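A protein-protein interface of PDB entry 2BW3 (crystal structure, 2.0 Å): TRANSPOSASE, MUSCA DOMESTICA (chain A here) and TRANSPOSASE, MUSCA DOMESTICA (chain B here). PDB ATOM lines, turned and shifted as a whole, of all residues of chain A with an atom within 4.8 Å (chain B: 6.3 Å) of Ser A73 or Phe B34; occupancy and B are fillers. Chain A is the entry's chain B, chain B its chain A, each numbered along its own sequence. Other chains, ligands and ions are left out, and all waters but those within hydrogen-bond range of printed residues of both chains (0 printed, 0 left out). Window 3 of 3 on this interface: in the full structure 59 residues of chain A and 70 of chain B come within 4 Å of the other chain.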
ATOM      1  N   PRO A  69      11.945   2.418   1.436  1.00  0.00           N
ATOM      2  CA  PRO A  69      10.641   1.757   1.533  1.00  0.00           C
ATOM      3  C   PRO A  69      10.755   0.330   2.090  1.00  0.00           C
ATOM      4  O   PRO A  69       9.992  -0.059   2.975  1.00  0.00           O
ATOM      5  CB  PRO A  69      10.152   1.770   0.078  1.00  0.00           C
ATOM      6  CG  PRO A  69      10.695   3.083  -0.428  1.00  0.00           C
ATOM      7  CD  PRO A  69      12.117   3.047   0.111  1.00  0.00           C
ATOM      8  N   ILE A  70      11.731  -0.444   1.614  1.00  0.00           N
ATOM      9  CA  ILE A  70      11.878  -1.807   2.125  1.00  0.00           C
ATOM     10  C   ILE A  70      12.222  -1.824   3.619  1.00  0.00           C
ATOM     11  O   ILE A  70      11.668  -2.608   4.389  1.00  0.00           O
ATOM     12  CB  ILE A  70      12.909  -2.627   1.297  1.00  0.00           C
ATOM     13  CG1 ILE A  70      12.824  -4.110   1.671  1.00  0.00           C
ATOM     14  CG2 ILE A  70      14.328  -2.098   1.513  1.00  0.00           C
ATOM     15  CD1 ILE A  70      13.562  -5.004   0.705  1.00  0.00           C
ATOM     16  N   THR A  71      13.077  -0.914   4.055  1.00  0.00           N
ATOM     17  CA  THR A  71      13.437  -0.873   5.469  1.00  0.00           C
ATOM     18  C   THR A  71      12.207  -0.525   6.313  1.00  0.00           C
ATOM     19  O   THR A  71      12.020  -1.047   7.411  1.00  0.00           O
ATOM     20  CB  THR A  71      14.553   0.166   5.737  1.00  0.00           C
ATOM     21  OG1 THR A  71      15.741  -0.186   5.000  1.00  0.00           O
ATOM     22  CG2 THR A  71      14.864   0.255   7.234  1.00  0.00           C
ATOM     23  N   LEU A  72      11.372   0.371   5.788  1.00  0.00           N
ATOM     24  CA  LEU A  72      10.162   0.793   6.481  1.00  0.00           C
ATOM     25  C   LEU A  72       9.147  -0.363   6.532  1.00  0.00           C
ATOM     26  O   LEU A  72       8.509  -0.600   7.561  1.00  0.00           O
ATOM     27  CB  LEU A  72       9.560   2.015   5.749  1.00  0.00           C
ATOM     28  CG  LEU A  72       8.362   2.669   6.429  1.00  0.00           C
ATOM     29  CD1 LEU A  72       8.718   3.067   7.856  1.00  0.00           C
ATOM     30  CD2 LEU A  72       7.929   3.892   5.614  1.00  0.00           C
ATOM     31  N   SER A  73       8.981  -1.049   5.407  1.00  0.00           N
ATOM     32  CA  SER A  73       8.064  -2.174   5.329  1.00  0.00           C
ATOM     33  C   SER A  73       8.471  -3.186   6.407  1.00  0.00           C
ATOM     34  O   SER A  73       7.641  -3.640   7.192  1.00  0.00           O
ATOM     35  CB  SER A  73       8.162  -2.830   3.950  1.00  0.00           C
ATOM     36  OG  SER A  73       7.092  -3.738   3.729  1.00  0.00           O
ATOM     37  N   ARG A  74       9.768  -3.489   6.473  1.00  0.00           N
ATOM     38  CA  ARG A  74      10.280  -4.454   7.447  1.00  0.00           C
ATOM     39  C   ARG A  74       9.997  -3.999   8.864  1.00  0.00           C
ATOM     40  O   ARG A  74       9.660  -4.814   9.732  1.00  0.00           O
ATOM     41  CB  ARG A  74      11.787  -4.704   7.240  1.00  0.00           C
ATOM     42  CG  ARG A  74      12.093  -5.440   5.945  1.00  0.00           C
ATOM     43  CD  ARG A  74      13.580  -5.599   5.698  1.00  0.00           C
ATOM     44  NE  ARG A  74      13.838  -6.518   4.591  1.00  0.00           N
ATOM     45  CZ  ARG A  74      14.787  -6.346   3.672  1.00  0.00           C
ATOM     46  NH1 ARG A  74      15.577  -5.281   3.718  1.00  0.00           N
ATOM     47  NH2 ARG A  74      14.938  -7.234   2.696  1.00  0.00           N
ATOM     48  N   LYS A  75      10.095  -2.693   9.089  1.00  0.00           N
ATOM     49  CA  LYS A  75       9.831  -2.148  10.408  1.00  0.00           C
ATOM     50  C   LYS A  75       8.356  -2.326  10.781  1.00  0.00           C
ATOM     51  O   LYS A  75       8.035  -2.738  11.896  1.00  0.00           O
ATOM     52  CB  LYS A  75      10.232  -0.667  10.462  1.00  0.00           C
ATOM     53  CG  LYS A  75       9.709   0.092  11.666  1.00  0.00           C
ATOM     54  CD  LYS A  75      10.241  -0.438  12.978  1.00  0.00           C
ATOM     55  CE  LYS A  75       9.868   0.513  14.100  1.00  0.00           C
ATOM     56  NZ  LYS A  75      10.372   0.055  15.422  1.00  0.00           N
ATOM     57  N   VAL A  76       7.464  -2.043   9.840  1.00  0.00           N
ATOM     58  CA  VAL A  76       6.029  -2.167  10.088  1.00  0.00           C
ATOM     59  C   VAL A  76       5.668  -3.640  10.334  1.00  0.00           C
ATOM     60  O   VAL A  76       4.895  -3.960  11.240  1.00  0.00           O
ATOM     61  CB  VAL A  76       5.227  -1.551   8.909  1.00  0.00           C
ATOM     62  CG1 VAL A  76       3.742  -1.890   9.012  1.00  0.00           C
ATOM     63  CG2 VAL A  76       5.413  -0.045   8.912  1.00  0.00           C
ATOM     64  N   THR A  77       6.276  -4.529   9.557  1.00  0.00           N
ATOM     65  CA  THR A  77       6.045  -5.965   9.704  1.00  0.00           C
ATOM     66  C   THR A  77       6.501  -6.500  11.063  1.00  0.00           C
ATOM     67  O   THR A  77       5.763  -7.254  11.699  1.00  0.00           O
ATOM     68  CB  THR A  77       6.721  -6.761   8.580  1.00  0.00           C
ATOM     69  OG1 THR A  77       6.077  -6.459   7.334  1.00  0.00           O
ATOM     70  CG2 THR A  77       6.616  -8.269   8.850  1.00  0.00           C
ATOM     71  N   VAL B  27       2.780   5.940   7.848  1.00  0.00           N
ATOM     72  CA  VAL B  27       2.195   5.021   6.863  1.00  0.00           C
ATOM     73  C   VAL B  27       1.087   4.116   7.401  1.00  0.00           C
ATOM     74  O   VAL B  27       0.150   3.785   6.674  1.00  0.00           O
ATOM     75  CB  VAL B  27       3.250   4.208   6.051  1.00  0.00           C
ATOM     76  CG1 VAL B  27       4.267   5.142   5.412  1.00  0.00           C
ATOM     77  CG2 VAL B  27       3.908   3.143   6.903  1.00  0.00           C
ATOM     78  N   VAL B  28       1.140   3.790   8.684  1.00  0.00           N
ATOM     79  CA  VAL B  28       0.126   2.939   9.285  1.00  0.00           C
ATOM     80  C   VAL B  28      -1.147   3.700   9.654  1.00  0.00           C
ATOM     81  O   VAL B  28      -2.236   3.345   9.222  1.00  0.00           O
ATOM     82  CB  VAL B  28       0.678   2.223  10.543  1.00  0.00           C
ATOM     83  CG1 VAL B  28      -0.481   1.524  11.298  1.00  0.00           C
ATOM     84  CG2 VAL B  28       1.739   1.190  10.139  1.00  0.00           C
ATOM     85  N   ARG B  32      -0.675   4.889   4.080  1.00  0.00           N
ATOM     86  CA  ARG B  32       0.088   5.361   2.921  1.00  0.00           C
ATOM     87  C   ARG B  32       1.015   4.246   2.459  1.00  0.00           C
ATOM     88  O   ARG B  32       1.418   3.405   3.246  1.00  0.00           O
ATOM     89  CB  ARG B  32       0.948   6.589   3.287  1.00  0.00           C
ATOM     90  CG  ARG B  32       0.151   7.856   3.662  1.00  0.00           C
ATOM     91  CD  ARG B  32      -0.825   8.353   2.553  1.00  0.00           C
ATOM     92  NE  ARG B  32      -1.750   9.340   3.125  1.00  0.00           N
ATOM     93  CZ  ARG B  32      -3.004   9.502   2.743  1.00  0.00           C
ATOM     94  NH1 ARG B  32      -3.505   8.768   1.755  1.00  0.00           N
ATOM     95  NH2 ARG B  32      -3.801  10.297   3.435  1.00  0.00           N
ATOM     96  N   PRO B  33       1.371   4.231   1.168  1.00  0.00           N
ATOM     97  CA  PRO B  33       2.269   3.163   0.708  1.00  0.00           C
ATOM     98  C   PRO B  33       3.709   3.402   1.172  1.00  0.00           C
ATOM     99  O   PRO B  33       4.123   4.545   1.387  1.00  0.00           O
ATOM    100  CB  PRO B  33       2.118   3.216  -0.816  1.00  0.00           C
ATOM    101  CG  PRO B  33       1.704   4.666  -1.086  1.00  0.00           C
ATOM    102  CD  PRO B  33       0.771   4.976   0.044  1.00  0.00           C
ATOM    103  N   PHE B  34       4.475   2.323   1.329  1.00  0.00           N
ATOM    104  CA  PHE B  34       5.858   2.423   1.787  1.00  0.00           C
ATOM    105  C   PHE B  34       6.693   3.274   0.851  1.00  0.00           C
ATOM    106  O   PHE B  34       7.577   3.992   1.292  1.00  0.00           O
ATOM    107  CB  PHE B  34       6.469   1.019   1.950  1.00  0.00           C
ATOM    108  CG  PHE B  34       5.772   0.184   2.998  1.00  0.00           C
ATOM    109  CD1 PHE B  34       5.146  -1.006   2.659  1.00  0.00           C
ATOM    110  CD2 PHE B  34       5.705   0.618   4.323  1.00  0.00           C
ATOM    111  CE1 PHE B  34       4.453  -1.751   3.637  1.00  0.00           C
ATOM    112  CE2 PHE B  34       5.025  -0.109   5.289  1.00  0.00           C
ATOM    113  CZ  PHE B  34       4.398  -1.292   4.952  1.00  0.00           C
ATOM    114  N   SER B  35       6.415   3.207  -0.446  1.00  0.00           N
ATOM    115  CA  SER B  35       7.150   4.014  -1.411  1.00  0.00           C
ATOM    116  C   SER B  35       7.011   5.528  -1.148  1.00  0.00           C
ATOM    117  O   SER B  35       7.825   6.324  -1.644  1.00  0.00           O
ATOM    118  CB  SER B  35       6.631   3.720  -2.810  1.00  0.00           C
ATOM    119  OG  SER B  35       5.259   4.068  -2.903  1.00  0.00           O
ATOM    120  N   ALA B  36       5.981   5.941  -0.403  1.00  0.00           N
ATOM    121  CA  ALA B  36       5.791   7.376  -0.127  1.00  0.00           C
ATOM    122  C   ALA B  36       6.992   8.032   0.564  1.00  0.00           C
ATOM    123  O   ALA B  36       7.263   9.229   0.368  1.00  0.00           O
ATOM    124  CB  ALA B  36       4.537   7.607   0.707  1.00  0.00           C
ATOM    125  N   VAL B  37       7.739   7.249   1.335  1.00  0.00           N
ATOM    126  CA  VAL B  37       8.869   7.797   2.074  1.00  0.00           C
ATOM    127  C   VAL B  37      10.095   8.070   1.185  1.00  0.00           C
ATOM    128  O   VAL B  37      11.003   8.788   1.577  1.00  0.00           O
ATOM    129  CB  VAL B  37       9.202   6.842   3.284  1.00  0.00           C
ATOM    130  CG1 VAL B  37       9.967   5.613   2.803  1.00  0.00           C
ATOM    131  CG2 VAL B  37       9.921   7.564   4.369  1.00  0.00           C
ATOM    132  N   SER B  38      10.072   7.535  -0.035  1.00  0.00           N
ATOM    133  CA  SER B  38      11.157   7.665  -0.998  1.00  0.00           C
ATOM    134  C   SER B  38      10.940   8.759  -2.065  1.00  0.00           C
ATOM    135  O   SER B  38      11.863   9.087  -2.818  1.00  0.00           O
ATOM    136  CB  SER B  38      11.309   6.312  -1.724  1.00  0.00           C
ATOM    137  OG  SER B  38      12.530   6.254  -2.405  1.00  0.00           O
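Pro A69 touches Phe B34 (CB to O, 3.6 Å).
Pro A69 touches Ser B35 (CG to CA, 3.8 Å).
Val B37 touches Pro A69 (CG1 to N, 3.999 Å).
Ser B38 touches Pro A69.
CG1 of Val B27 touches CD2 of Leu A72 (3.9 Å).
CG of Leu A72 touches CD2 of Phe B34, 3.96 Å away.
Val B37 touches Leu A72 (CG1 to CD2, 3.9 Å).
Ser A73 touches Phe B34.
CG1 of Val A76 touches CG2 of Val B28 (3.8 Å).
Val A76 touches Phe B34 (CG2 to CE2, 3.6 Å).
Printed residues of chain B that touch a printed residue of chain A: Val B27, Val B28, Phe B34, Ser B35, Val B37 and Ser B38.
Hydrophobic or aromatic side chains of chain B that line the printed part of chain A: Val B27, Val B28, Phe B34 and Val B37.
Hydrophobic or aromatic side chains of chain A within 4 Å of the printed part of chain B: Pro A69, Leu A72 and Val A76.
Along chain A the printed residues that touch a printed residue of chain B span positions 69 to 76.
Among the printed residues, 10 pairs touch across the chains.
Among the printed residues, no Asp or Glu carboxylate lies within 4 Å of a Lys or Arg side-chain nitrogen of the other chain.
Ile A70 touches none of the printed residues of chain B.
Of the printed residues of chain B, Leu A72 touches Val B27 (3.9 Å), Phe B34 (3.96 Å) and Val B37 (3.9 Å).
Of chain B, only Phe B34 comes within 4 Å of Ser A73.
Of the printed residues of chain B, Val A76 touches Val B28 and Phe B34.
Printed residues of chain A within 4 Å of Val B28: Val A76 (3.8 Å).
Pro B33 touches none of the printed residues of chain A.
Phe B34 touches just these residues of chain A: Pro A69 (3.6 Å), Leu A72 (3.96 Å), Ser A73 (3.3 Å) and Val A76 (3.6 Å).
Printed residues of chain A within 4 Å of Val B37: Pro A69 and Leu A72.
Of the printed residues of chain A, Ser B38 touches Pro A69 (3.5 Å).
The nearest printed residue of chain B that does not touch Pro A69 is Ala B36 (5.5 Å).
The backbone carbonyl oxygen (O) of Val B27 sits at hydrogen-bond distance from the backbone NH (N) of Arg B32 (2.9 Å).
The side-chain hydroxyl (OG1) of Thr A77 lies within hydrogen-bond range of the backbone carbonyl oxygen (O) of Ser A73.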
